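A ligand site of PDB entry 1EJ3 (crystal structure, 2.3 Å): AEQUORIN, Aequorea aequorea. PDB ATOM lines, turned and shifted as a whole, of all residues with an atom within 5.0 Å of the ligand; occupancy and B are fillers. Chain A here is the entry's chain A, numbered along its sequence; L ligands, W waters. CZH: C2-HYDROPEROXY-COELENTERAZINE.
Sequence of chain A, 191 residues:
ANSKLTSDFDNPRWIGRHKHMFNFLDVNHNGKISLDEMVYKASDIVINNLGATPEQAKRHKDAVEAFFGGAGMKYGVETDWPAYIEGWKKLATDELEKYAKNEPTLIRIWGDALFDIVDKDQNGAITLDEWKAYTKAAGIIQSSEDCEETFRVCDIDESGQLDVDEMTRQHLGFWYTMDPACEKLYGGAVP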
ATOM      1  N   HIS A  18      -9.437 -27.191   8.680  1.00  0.00           N
ATOM      2  CA  HIS A  18      -9.330 -25.898   9.331  1.00  0.00           C
ATOM      3  C   HIS A  18      -8.323 -25.871  10.488  1.00  0.00           C
ATOM      4  O   HIS A  18      -7.823 -24.818  10.847  1.00  0.00           O
ATOM      5  CB  HIS A  18     -10.708 -25.431   9.771  1.00  0.00           C
ATOM      6  CG  HIS A  18     -11.578 -25.038   8.625  1.00  0.00           C
ATOM      7  ND1 HIS A  18     -11.384 -23.871   7.914  1.00  0.00           N
ATOM      8  CD2 HIS A  18     -12.568 -25.704   7.988  1.00  0.00           C
ATOM      9  CE1 HIS A  18     -12.223 -23.837   6.895  1.00  0.00           C
ATOM     10  NE2 HIS A  18     -12.951 -24.932   6.916  1.00  0.00           N
ATOM     11  N   MET A  21      -5.144 -25.184   8.734  1.00  0.00           N
ATOM     12  CA  MET A  21      -5.074 -23.780   8.386  1.00  0.00           C
ATOM     13  C   MET A  21      -4.807 -22.921   9.613  1.00  0.00           C
ATOM     14  O   MET A  21      -4.020 -21.987   9.557  1.00  0.00           O
ATOM     15  CB  MET A  21      -6.360 -23.337   7.690  1.00  0.00           C
ATOM     16  CG  MET A  21      -6.521 -23.902   6.282  1.00  0.00           C
ATOM     17  SD  MET A  21      -5.049 -23.655   5.242  1.00  0.00           S
ATOM     18  CE  MET A  21      -5.053 -21.885   5.091  1.00  0.00           C
ATOM     19  N   PHE A  24      -1.275 -23.164  10.377  1.00  0.00           N
ATOM     20  CA  PHE A  24      -0.506 -22.489   9.325  1.00  0.00           C
ATOM     21  C   PHE A  24      -0.495 -20.986   9.609  1.00  0.00           C
ATOM     22  O   PHE A  24       0.505 -20.312   9.420  1.00  0.00           O
ATOM     23  CB  PHE A  24      -1.153 -22.771   7.965  1.00  0.00           C
ATOM     24  CG  PHE A  24      -0.821 -21.751   6.903  1.00  0.00           C
ATOM     25  CD1 PHE A  24       0.447 -21.715   6.318  1.00  0.00           C
ATOM     26  CD2 PHE A  24      -1.787 -20.846   6.459  1.00  0.00           C
ATOM     27  CE1 PHE A  24       0.743 -20.789   5.305  1.00  0.00           C
ATOM     28  CE2 PHE A  24      -1.496 -19.914   5.458  1.00  0.00           C
ATOM     29  CZ  PHE A  24      -0.232 -19.887   4.876  1.00  0.00           C
ATOM     30  N   LEU A  25      -1.628 -20.474  10.067  1.00  0.00           N
ATOM     31  CA  LEU A  25      -1.770 -19.055  10.373  1.00  0.00           C
ATOM     32  C   LEU A  25      -1.110 -18.665  11.700  1.00  0.00           C
ATOM     33  O   LEU A  25      -0.655 -17.526  11.835  1.00  0.00           O
ATOM     34  CB  LEU A  25      -3.255 -18.664  10.391  1.00  0.00           C
ATOM     35  CG  LEU A  25      -4.013 -18.797   9.064  1.00  0.00           C
ATOM     36  CD1 LEU A  25      -5.514 -18.575   9.277  1.00  0.00           C
ATOM     37  CD2 LEU A  25      -3.473 -17.788   8.074  1.00  0.00           C
ATOM     38  N   MET A  38      -4.032 -11.396  10.518  1.00  0.00           N
ATOM     39  CA  MET A  38      -4.603 -11.841   9.247  1.00  0.00           C
ATOM     40  C   MET A  38      -4.560 -10.771   8.164  1.00  0.00           C
ATOM     41  O   MET A  38      -4.177 -11.026   7.015  1.00  0.00           O
ATOM     42  CB  MET A  38      -6.049 -12.278   9.468  1.00  0.00           C
ATOM     43  CG  MET A  38      -6.211 -13.395  10.491  1.00  0.00           C
ATOM     44  SD  MET A  38      -5.278 -14.877  10.030  1.00  0.00           S
ATOM     45  CE  MET A  38      -3.689 -14.570  10.861  1.00  0.00           C
ATOM     46  N   LYS A  41      -0.928  -9.990   7.227  1.00  0.00           N
ATOM     47  CA  LYS A  41      -0.436 -11.001   6.319  1.00  0.00           C
ATOM     48  C   LYS A  41      -0.987 -10.821   4.902  1.00  0.00           C
ATOM     49  O   LYS A  41      -0.256 -10.954   3.937  1.00  0.00           O
ATOM     50  CB  LYS A  41      -0.801 -12.390   6.847  1.00  0.00           C
ATOM     51  CG  LYS A  41      -0.440 -13.549   5.901  1.00  0.00           C
ATOM     52  CD  LYS A  41      -0.905 -14.883   6.464  1.00  0.00           C
ATOM     53  CE  LYS A  41      -0.716 -16.039   5.468  1.00  0.00           C
ATOM     54  NZ  LYS A  41       0.696 -16.470   5.331  1.00  0.00           N
ATOM     55  N   ALA A  42      -2.271 -10.497   4.802  1.00  0.00           N
ATOM     56  CA  ALA A  42      -2.919 -10.278   3.517  1.00  0.00           C
ATOM     57  C   ALA A  42      -2.293  -9.130   2.730  1.00  0.00           C
ATOM     58  O   ALA A  42      -1.939  -9.277   1.561  1.00  0.00           O
ATOM     59  CB  ALA A  42      -4.405 -10.022   3.718  1.00  0.00           C
ATOM     60  N   ILE A  45       1.557  -9.638   1.716  1.00  0.00           N
ATOM     61  CA  ILE A  45       1.658 -10.474   0.535  1.00  0.00           C
ATOM     62  C   ILE A  45       1.403  -9.720  -0.779  1.00  0.00           C
ATOM     63  O   ILE A  45       2.232  -9.739  -1.679  1.00  0.00           O
ATOM     64  CB  ILE A  45       0.653 -11.661   0.600  1.00  0.00           C
ATOM     65  CG1 ILE A  45       1.031 -12.604   1.734  1.00  0.00           C
ATOM     66  CG2 ILE A  45       0.606 -12.400  -0.731  1.00  0.00           C
ATOM     67  CD1 ILE A  45      -0.058 -13.581   2.100  1.00  0.00           C
ATOM     68  N   VAL A  64     -10.426  -9.427   3.044  1.00  0.00           N
ATOM     69  CA  VAL A  64      -9.840 -10.341   4.020  1.00  0.00           C
ATOM     70  C   VAL A  64     -10.405 -10.064   5.418  1.00  0.00           C
ATOM     71  O   VAL A  64     -10.662 -10.980   6.193  1.00  0.00           O
ATOM     72  CB  VAL A  64      -8.292 -10.193   4.071  1.00  0.00           C
ATOM     73  CG1 VAL A  64      -7.704 -11.060   5.198  1.00  0.00           C
ATOM     74  CG2 VAL A  64      -7.709 -10.596   2.731  1.00  0.00           C
ATOM     75  N   PHE A  67     -13.832 -11.428   5.683  1.00  0.00           N
ATOM     76  CA  PHE A  67     -13.737 -12.870   5.706  1.00  0.00           C
ATOM     77  C   PHE A  67     -13.512 -13.412   7.111  1.00  0.00           C
ATOM     78  O   PHE A  67     -14.357 -14.148   7.643  1.00  0.00           O
ATOM     79  CB  PHE A  67     -12.608 -13.331   4.793  1.00  0.00           C
ATOM     80  CG  PHE A  67     -12.540 -14.822   4.620  1.00  0.00           C
ATOM     81  CD1 PHE A  67     -13.515 -15.503   3.884  1.00  0.00           C
ATOM     82  CD2 PHE A  67     -11.493 -15.557   5.178  1.00  0.00           C
ATOM     83  CE1 PHE A  67     -13.442 -16.894   3.713  1.00  0.00           C
ATOM     84  CE2 PHE A  67     -11.419 -16.948   5.007  1.00  0.00           C
ATOM     85  CZ  PHE A  67     -12.400 -17.615   4.271  1.00  0.00           C
ATOM     86  N   PHE A  68     -12.398 -13.056   7.728  1.00  0.00           N
ATOM     87  CA  PHE A  68     -12.098 -13.535   9.076  1.00  0.00           C
ATOM     88  C   PHE A  68     -13.008 -12.919  10.136  1.00  0.00           C
ATOM     89  O   PHE A  68     -13.126 -13.435  11.255  1.00  0.00           O
ATOM     90  CB  PHE A  68     -10.618 -13.316   9.404  1.00  0.00           C
ATOM     91  CG  PHE A  68      -9.692 -14.199   8.598  1.00  0.00           C
ATOM     92  CD1 PHE A  68      -9.156 -13.769   7.387  1.00  0.00           C
ATOM     93  CD2 PHE A  68      -9.403 -15.497   9.022  1.00  0.00           C
ATOM     94  CE1 PHE A  68      -8.352 -14.597   6.623  1.00  0.00           C
ATOM     95  CE2 PHE A  68      -8.603 -16.335   8.261  1.00  0.00           C
ATOM     96  CZ  PHE A  68      -8.072 -15.891   7.050  1.00  0.00           C
ATOM     97  N   TYR A  84     -12.164 -20.249  17.273  1.00  0.00           N
ATOM     98  CA  TYR A  84     -11.909 -20.196  15.846  1.00  0.00           C
ATOM     99  C   TYR A  84     -12.785 -21.167  15.042  1.00  0.00           C
ATOM    100  O   TYR A  84     -13.475 -20.773  14.115  1.00  0.00           O
ATOM    101  CB  TYR A  84     -10.434 -20.490  15.580  1.00  0.00           C
ATOM    102  CG  TYR A  84     -10.049 -20.368  14.120  1.00  0.00           C
ATOM    103  CD1 TYR A  84      -9.890 -19.125  13.525  1.00  0.00           C
ATOM    104  CD2 TYR A  84      -9.869 -21.509  13.338  1.00  0.00           C
ATOM    105  CE1 TYR A  84      -9.564 -19.012  12.171  1.00  0.00           C
ATOM    106  CE2 TYR A  84      -9.550 -21.414  11.989  1.00  0.00           C
ATOM    107  CZ  TYR A  84      -9.385 -20.168  11.413  1.00  0.00           C
ATOM    108  OH  TYR A  84      -9.060 -20.069  10.083  1.00  0.00           O
ATOM    109  N   TRP A  88     -15.933 -20.557  12.767  1.00  0.00           N
ATOM    110  CA  TRP A  88     -15.915 -20.981  11.371  1.00  0.00           C
ATOM    111  C   TRP A  88     -17.233 -21.644  10.938  1.00  0.00           C
ATOM    112  O   TRP A  88     -17.608 -21.575   9.770  1.00  0.00           O
ATOM    113  CB  TRP A  88     -14.744 -21.930  11.093  1.00  0.00           C
ATOM    114  CG  TRP A  88     -13.716 -21.311  10.189  1.00  0.00           C
ATOM    115  CD1 TRP A  88     -12.607 -20.622  10.559  1.00  0.00           C
ATOM    116  CD2 TRP A  88     -13.755 -21.268   8.755  1.00  0.00           C
ATOM    117  NE1 TRP A  88     -11.953 -20.143   9.451  1.00  0.00           N
ATOM    118  CE2 TRP A  88     -12.638 -20.525   8.334  1.00  0.00           C
ATOM    119  CE3 TRP A  88     -14.640 -21.776   7.790  1.00  0.00           C
ATOM    120  CZ2 TRP A  88     -12.368 -20.275   6.975  1.00  0.00           C
ATOM    121  CZ3 TRP A  88     -14.372 -21.533   6.443  1.00  0.00           C
ATOM    122  CH2 TRP A  88     -13.245 -20.785   6.050  1.00  0.00           C
ATOM    123  N   ILE A 107     -15.948 -15.130   0.325  1.00  0.00           N
ATOM    124  CA  ILE A 107     -14.839 -15.761  -0.361  1.00  0.00           C
ATOM    125  C   ILE A 107     -14.798 -15.298  -1.829  1.00  0.00           C
ATOM    126  O   ILE A 107     -13.722 -15.159  -2.422  1.00  0.00           O
ATOM    127  CB  ILE A 107     -14.912 -17.314  -0.275  1.00  0.00           C
ATOM    128  CG1 ILE A 107     -13.683 -17.951  -0.924  1.00  0.00           C
ATOM    129  CG2 ILE A 107     -16.166 -17.822  -0.958  1.00  0.00           C
ATOM    130  CD1 ILE A 107     -12.391 -17.492  -0.309  1.00  0.00           C
ATOM    131  N   TRP A 110     -13.275 -11.851  -1.970  1.00  0.00           N
ATOM    132  CA  TRP A 110     -11.837 -11.962  -1.776  1.00  0.00           C
ATOM    133  C   TRP A 110     -11.178 -12.337  -3.103  1.00  0.00           C
ATOM    134  O   TRP A 110     -10.260 -11.653  -3.554  1.00  0.00           O
ATOM    135  CB  TRP A 110     -11.531 -13.050  -0.731  1.00  0.00           C
ATOM    136  CG  TRP A 110     -10.075 -13.160  -0.329  1.00  0.00           C
ATOM    137  CD1 TRP A 110      -9.013 -12.464  -0.830  1.00  0.00           C
ATOM    138  CD2 TRP A 110      -9.532 -14.035   0.676  1.00  0.00           C
ATOM    139  NE1 TRP A 110      -7.850 -12.844  -0.211  1.00  0.00           N
ATOM    140  CE2 TRP A 110      -8.141 -13.809   0.722  1.00  0.00           C
ATOM    141  CE3 TRP A 110     -10.088 -14.995   1.546  1.00  0.00           C
ATOM    142  CZ2 TRP A 110      -7.292 -14.495   1.594  1.00  0.00           C
ATOM    143  CZ3 TRP A 110      -9.239 -15.681   2.417  1.00  0.00           C
ATOM    144  CH2 TRP A 110      -7.851 -15.427   2.439  1.00  0.00           C
ATOM    145  N   GLY A 111     -11.669 -13.407  -3.718  1.00  0.00           N
ATOM    146  CA  GLY A 111     -11.130 -13.860  -4.993  1.00  0.00           C
ATOM    147  C   GLY A 111     -11.037 -12.746  -6.013  1.00  0.00           C
ATOM    148  O   GLY A 111      -9.981 -12.570  -6.627  1.00  0.00           O
ATOM    149  N   LEU A 114      -8.252 -10.417  -5.036  1.00  0.00           N
ATOM    150  CA  LEU A 114      -6.955 -11.038  -5.252  1.00  0.00           C
ATOM    151  C   LEU A 114      -6.585 -11.261  -6.712  1.00  0.00           C
ATOM    152  O   LEU A 114      -5.446 -10.983  -7.104  1.00  0.00           O
ATOM    153  CB  LEU A 114      -6.871 -12.364  -4.478  1.00  0.00           C
ATOM    154  CG  LEU A 114      -5.521 -13.086  -4.544  1.00  0.00           C
ATOM    155  CD1 LEU A 114      -4.432 -12.191  -3.979  1.00  0.00           C
ATOM    156  CD2 LEU A 114      -5.595 -14.386  -3.764  1.00  0.00           C
ATOM    157  N   PHE A 115      -7.524 -11.750  -7.513  1.00  0.00           N
ATOM    158  CA  PHE A 115      -7.246 -12.013  -8.937  1.00  0.00           C
ATOM    159  C   PHE A 115      -6.947 -10.743  -9.721  1.00  0.00           C
ATOM    160  O   PHE A 115      -6.230 -10.772 -10.732  1.00  0.00           O
ATOM    161  CB  PHE A 115      -8.419 -12.761  -9.585  1.00  0.00           C
ATOM    162  CG  PHE A 115      -8.369 -14.257  -9.400  1.00  0.00           C
ATOM    163  CD1 PHE A 115      -8.254 -14.815  -8.126  1.00  0.00           C
ATOM    164  CD2 PHE A 115      -8.489 -15.116 -10.494  1.00  0.00           C
ATOM    165  CE1 PHE A 115      -8.255 -16.202  -7.954  1.00  0.00           C
ATOM    166  CE2 PHE A 115      -8.498 -16.491 -10.331  1.00  0.00           C
ATOM    167  CZ  PHE A 115      -8.387 -17.036  -9.058  1.00  0.00           C
ATOM    168  N   TRP A 131      -0.532 -18.501 -10.165  1.00  0.00           N
ATOM    169  CA  TRP A 131      -1.115 -19.232  -9.037  1.00  0.00           C
ATOM    170  C   TRP A 131       0.013 -19.631  -8.093  1.00  0.00           C
ATOM    171  O   TRP A 131      -0.114 -19.519  -6.865  1.00  0.00           O
ATOM    172  CB  TRP A 131      -1.849 -20.475  -9.532  1.00  0.00           C
ATOM    173  CG  TRP A 131      -2.469 -21.321  -8.458  1.00  0.00           C
ATOM    174  CD1 TRP A 131      -2.343 -22.669  -8.312  1.00  0.00           C
ATOM    175  CD2 TRP A 131      -3.328 -20.874  -7.397  1.00  0.00           C
ATOM    176  NE1 TRP A 131      -3.083 -23.099  -7.237  1.00  0.00           N
ATOM    177  CE2 TRP A 131      -3.703 -22.024  -6.661  1.00  0.00           C
ATOM    178  CE3 TRP A 131      -3.825 -19.628  -7.008  1.00  0.00           C
ATOM    179  CZ2 TRP A 131      -4.547 -21.954  -5.551  1.00  0.00           C
ATOM    180  CZ3 TRP A 131      -4.668 -19.551  -5.910  1.00  0.00           C
ATOM    181  CH2 TRP A 131      -5.021 -20.715  -5.190  1.00  0.00           C
ATOM    182  N   TYR A 134       1.369 -16.609  -6.133  1.00  0.00           N
ATOM    183  CA  TYR A 134       0.525 -16.266  -4.985  1.00  0.00           C
ATOM    184  C   TYR A 134       0.587 -17.304  -3.868  1.00  0.00           C
ATOM    185  O   TYR A 134       0.892 -16.962  -2.715  1.00  0.00           O
ATOM    186  CB  TYR A 134      -0.937 -16.099  -5.394  1.00  0.00           C
ATOM    187  CG  TYR A 134      -1.824 -16.025  -4.186  1.00  0.00           C
ATOM    188  CD1 TYR A 134      -1.755 -14.931  -3.318  1.00  0.00           C
ATOM    189  CD2 TYR A 134      -2.631 -17.095  -3.833  1.00  0.00           C
ATOM    190  CE1 TYR A 134      -2.463 -14.921  -2.137  1.00  0.00           C
ATOM    191  CE2 TYR A 134      -3.340 -17.092  -2.640  1.00  0.00           C
ATOM    192  CZ  TYR A 134      -3.243 -16.005  -1.790  1.00  0.00           C
ATOM    193  OH  TYR A 134      -3.894 -16.033  -0.578  1.00  0.00           O
ATOM    194  N   ALA A 138       2.104 -16.651  -0.085  1.00  0.00           N
ATOM    195  CA  ALA A 138       1.276 -16.768   1.105  1.00  0.00           C
ATOM    196  C   ALA A 138       1.726 -17.956   1.959  1.00  0.00           C
ATOM    197  O   ALA A 138       1.561 -17.963   3.188  1.00  0.00           O
ATOM    198  CB  ALA A 138      -0.183 -16.938   0.709  1.00  0.00           C
ATOM    199  N   ILE A 140       0.549 -21.060   1.575  1.00  0.00           N
ATOM    200  CA  ILE A 140      -0.476 -22.097   1.621  1.00  0.00           C
ATOM    201  C   ILE A 140      -0.078 -23.334   0.804  1.00  0.00           C
ATOM    202  O   ILE A 140      -0.550 -24.428   1.072  1.00  0.00           O
ATOM    203  CB  ILE A 140      -1.836 -21.541   1.143  1.00  0.00           C
ATOM    204  CG1 ILE A 140      -2.930 -22.577   1.425  1.00  0.00           C
ATOM    205  CG2 ILE A 140      -1.766 -21.158  -0.322  1.00  0.00           C
ATOM    206  CD1 ILE A 140      -4.311 -22.004   1.442  1.00  0.00           C
ATOM    207  N   VAL A 164     -11.837 -17.022 -11.698  1.00  0.00           N
ATOM    208  CA  VAL A 164     -12.399 -16.755 -10.363  1.00  0.00           C
ATOM    209  C   VAL A 164     -13.732 -17.458 -10.113  1.00  0.00           C
ATOM    210  O   VAL A 164     -14.008 -17.934  -9.013  1.00  0.00           O
ATOM    211  CB  VAL A 164     -12.648 -15.260 -10.141  1.00  0.00           C
ATOM    212  CG1 VAL A 164     -12.639 -14.950  -8.672  1.00  0.00           C
ATOM    213  CG2 VAL A 164     -11.636 -14.435 -10.883  1.00  0.00           C
ATOM    214  N   MET A 167     -12.860 -21.118  -9.499  1.00  0.00           N
ATOM    215  CA  MET A 167     -12.189 -21.292  -8.219  1.00  0.00           C
ATOM    216  C   MET A 167     -13.166 -21.073  -7.070  1.00  0.00           C
ATOM    217  O   MET A 167     -13.113 -21.788  -6.058  1.00  0.00           O
ATOM    218  CB  MET A 167     -11.008 -20.332  -8.079  1.00  0.00           C
ATOM    219  CG  MET A 167     -10.174 -20.606  -6.857  1.00  0.00           C
ATOM    220  SD  MET A 167      -9.465 -22.301  -6.898  1.00  0.00           S
ATOM    221  CE  MET A 167      -7.770 -21.921  -6.445  1.00  0.00           C
ATOM    222  N   THR A 168     -14.051 -20.085  -7.213  1.00  0.00           N
ATOM    223  CA  THR A 168     -15.025 -19.810  -6.170  1.00  0.00           C
ATOM    224  C   THR A 168     -15.825 -21.086  -5.923  1.00  0.00           C
ATOM    225  O   THR A 168     -15.952 -21.559  -4.787  1.00  0.00           O
ATOM    226  CB  THR A 168     -16.019 -18.680  -6.589  1.00  0.00           C
ATOM    227  OG1 THR A 168     -15.302 -17.454  -6.789  1.00  0.00           O
ATOM    228  CG2 THR A 168     -17.082 -18.481  -5.515  1.00  0.00           C
ATOM    229  N   HIS A 171     -13.866 -23.482  -3.932  1.00  0.00           N
ATOM    230  CA  HIS A 171     -13.752 -23.092  -2.532  1.00  0.00           C
ATOM    231  C   HIS A 171     -15.008 -23.353  -1.710  1.00  0.00           C
ATOM    232  O   HIS A 171     -14.917 -23.691  -0.530  1.00  0.00           O
ATOM    233  CB  HIS A 171     -13.357 -21.614  -2.412  1.00  0.00           C
ATOM    234  CG  HIS A 171     -11.902 -21.369  -2.615  1.00  0.00           C
ATOM    235  ND1 HIS A 171     -11.380 -20.127  -2.849  1.00  0.00           N
ATOM    236  CD2 HIS A 171     -10.847 -22.234  -2.602  1.00  0.00           C
ATOM    237  CE1 HIS A 171     -10.067 -20.217  -2.979  1.00  0.00           C
ATOM    238  NE2 HIS A 171      -9.719 -21.492  -2.834  1.00  0.00           N
ATOM    239  N   TRP A 175     -13.728 -25.533   1.291  1.00  0.00           N
ATOM    240  CA  TRP A 175     -13.780 -24.943   2.626  1.00  0.00           C
ATOM    241  C   TRP A 175     -15.094 -25.048   3.398  1.00  0.00           C
ATOM    242  O   TRP A 175     -15.080 -25.087   4.627  1.00  0.00           O
ATOM    243  CB  TRP A 175     -13.401 -23.450   2.556  1.00  0.00           C
ATOM    244  CG  TRP A 175     -12.037 -23.173   2.005  1.00  0.00           C
ATOM    245  CD1 TRP A 175     -11.739 -22.409   0.912  1.00  0.00           C
ATOM    246  CD2 TRP A 175     -10.791 -23.656   2.519  1.00  0.00           C
ATOM    247  NE1 TRP A 175     -10.373 -22.386   0.713  1.00  0.00           N
ATOM    248  CE2 TRP A 175      -9.772 -23.135   1.688  1.00  0.00           C
ATOM    249  CE3 TRP A 175     -10.437 -24.468   3.607  1.00  0.00           C
ATOM    250  CZ2 TRP A 175      -8.421 -23.406   1.907  1.00  0.00           C
ATOM    251  CZ3 TRP A 175      -9.081 -24.729   3.823  1.00  0.00           C
ATOM    252  CH2 TRP A 175      -8.089 -24.204   2.968  1.00  0.00           C
ATOM    253  N   TYR A 186      -5.704 -28.153  -3.259  1.00  0.00           N
ATOM    254  CA  TYR A 186      -4.370 -27.628  -2.989  1.00  0.00           C
ATOM    255  C   TYR A 186      -3.365 -28.779  -2.911  1.00  0.00           C
ATOM    256  O   TYR A 186      -2.457 -28.745  -2.086  1.00  0.00           O
ATOM    257  CB  TYR A 186      -4.320 -26.851  -1.676  1.00  0.00           C
ATOM    258  CG  TYR A 186      -5.192 -25.631  -1.639  1.00  0.00           C
ATOM    259  CD1 TYR A 186      -6.587 -25.758  -1.626  1.00  0.00           C
ATOM    260  CD2 TYR A 186      -4.639 -24.357  -1.623  1.00  0.00           C
ATOM    261  CE1 TYR A 186      -7.410 -24.634  -1.610  1.00  0.00           C
ATOM    262  CE2 TYR A 186      -5.455 -23.223  -1.600  1.00  0.00           C
ATOM    263  CZ  TYR A 186      -6.832 -23.380  -1.588  1.00  0.00           C
ATOM    264  OH  TYR A 186      -7.644 -22.273  -1.541  1.00  0.00           O
HETATM  265  N1  CZH L   1      -5.572 -17.773   0.155  1.00  0.00           N
HETATM  266  C2  CZH L   1      -6.550 -18.031  -0.865  1.00  0.00           C
HETATM  267  C3  CZH L   1      -7.678 -18.790  -0.075  1.00  0.00           C
HETATM  268  N4  CZH L   1      -7.297 -18.890   1.182  1.00  0.00           N
HETATM  269  C5  CZH L   1      -8.037 -19.521   2.302  1.00  0.00           C
HETATM  270  C6  CZH L   1      -7.447 -19.515   3.536  1.00  0.00           C
HETATM  271  N7  CZH L   1      -6.105 -18.872   3.687  1.00  0.00           N
HETATM  272  C8  CZH L   1      -5.439 -18.294   2.654  1.00  0.00           C
HETATM  273  C9  CZH L   1      -6.082 -18.296   1.288  1.00  0.00           C
HETATM  274  C10 CZH L   1      -7.091 -16.691  -1.469  1.00  0.00           C
HETATM  275  C11 CZH L   1      -8.092 -16.880  -2.590  1.00  0.00           C
HETATM  276  C12 CZH L   1      -7.703 -17.419  -3.874  1.00  0.00           C
HETATM  277  C13 CZH L   1      -8.664 -17.596  -4.903  1.00  0.00           C
HETATM  278  C14 CZH L   1     -10.036 -17.243  -4.670  1.00  0.00           C
HETATM  279  C15 CZH L   1     -10.440 -16.703  -3.402  1.00  0.00           C
HETATM  280  C16 CZH L   1      -9.460 -16.518  -2.360  1.00  0.00           C
HETATM  281  O17 CZH L   1     -10.931 -17.417  -5.668  1.00  0.00           O
HETATM  282  O18 CZH L   1      -8.712 -19.202  -0.581  1.00  0.00           O
HETATM  283  C19 CZH L   1      -8.044 -20.120   4.721  1.00  0.00           C
HETATM  284  C20 CZH L   1      -7.679 -19.613   6.008  1.00  0.00           C
HETATM  285  C21 CZH L   1      -8.245 -20.216   7.172  1.00  0.00           C
HETATM  286  C22 CZH L   1      -9.144 -21.312   7.059  1.00  0.00           C
HETATM  287  C23 CZH L   1      -9.503 -21.816   5.791  1.00  0.00           C
HETATM  288  C24 CZH L   1      -8.966 -21.231   4.639  1.00  0.00           C
HETATM  289  O25 CZH L   1      -9.648 -21.871   8.195  1.00  0.00           O
HETATM  290  C26 CZH L   1      -4.072 -17.673   2.950  1.00  0.00           C
HETATM  291  C27 CZH L   1      -4.162 -16.316   3.602  1.00  0.00           C
HETATM  292  C28 CZH L   1      -3.731 -15.154   2.877  1.00  0.00           C
HETATM  293  C29 CZH L   1      -3.802 -13.853   3.489  1.00  0.00           C
HETATM  294  C30 CZH L   1      -4.290 -13.709   4.821  1.00  0.00           C
HETATM  295  C31 CZH L   1      -4.721 -14.872   5.545  1.00  0.00           C
HETATM  296  C32 CZH L   1      -4.656 -16.167   4.945  1.00  0.00           C
HETATM  297  O33 CZH L   1      -5.844 -18.795  -1.885  1.00  0.00           O
HETATM  298  O34 CZH L   1      -6.310 -20.129  -2.080  1.00  0.00           O
HETATM  299  O   HOH W   1      -4.676 -13.238   0.153  1.00  0.00           O
HETATM  300  O   HOH W   2     -13.587 -17.389  -4.455  1.00  0.00           O
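OH of Tyr 84 lies within hydrogen-bond range of NE1 of Trp 88, at 3.0 Å. The backbone carbonyl oxygen (O) of Ala 138 is in hydrogen-bond range of the side-chain amino group (NZ) of Lys 41, at 2.8 Å. A ring nitrogen (NE2) of His 171 lies within hydrogen-bond range of the side-chain hydroxyl of Tyr 186, at 2.6 Å. O of Trp 175 is in hydrogen-bond range of NE2 of His 18 (3.1 Å).
The side-chain hydroxyl of Tyr 186 lies within hydrogen-bond range of an oxygen (O34) of the ligand (2.6 Å). A ring nitrogen (NE2) of His 171 lies close to an oxygen (O18) of the ligand (3.4 Å). A nitrogen (N1) of the ligand sits at hydrogen-bond distance from the side-chain hydroxyl (OH) of Tyr 134 (2.5 Å). An oxygen (O25) of the ligand sits at hydrogen-bond distance from the side-chain hydroxyl of Tyr 84. O25 of the ligand sits at hydrogen-bond distance from ND1 of His 18 (2.7 Å). NE1 of Trp 88 lies within hydrogen-bond range of O25 of the ligand.
Water W2 lies within hydrogen-bond range of the side-chain hydroxyl (OG1) of Thr 168 (2.9 Å), an oxygen (O17) of the ligand (2.9 Å) and the backbone carbonyl oxygen (O) of Ile 107 (3.0 Å). Water W1 lies within hydrogen-bond range of the side-chain hydroxyl (OH) of Tyr 134 (3.0 Å) and the indole nitrogen (NE1) of Trp 110 (3.2 Å).
Residues that only touch the ligand: Gly 111 (3.3 Å), Phe 115 (3.4 Å), Trp 131 (3.4 Å), Met 38 (3.5 Å), Met 21 (3.5 Å), Met 167 (3.5 Å), Trp 175 (3.5 Å), Trp 110 (3.6 Å), Leu 114 (3.6 Å), Ala 42 (3.7 Å), Ile 107 (3.7 Å), Leu 25 (3.7 Å), Phe 68 (3.8 Å) and Lys 41 (3.9 Å). Hydrophobic or aromatic side chains within 4 Å of the ligand: His 18, Met 21, Leu 25, Ala 42, Phe 68, Tyr 84, Trp 88, Ile 107, Trp 110, Leu 114, Phe 115, Trp 131, Tyr 134, Met 167, His 171, Trp 175 and Tyr 186. 20 residues have an atom within 4 Å of the ligand: His 18, Met 21, Leu 25, Met 38, Lys 41, Ala 42, Phe 68, Tyr 84, Trp 88, Ile 107, Trp 110, Gly 111, Leu 114, Phe 115, Trp 131, Tyr 134, Met 167, His 171, Trp 175 and Tyr 186.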
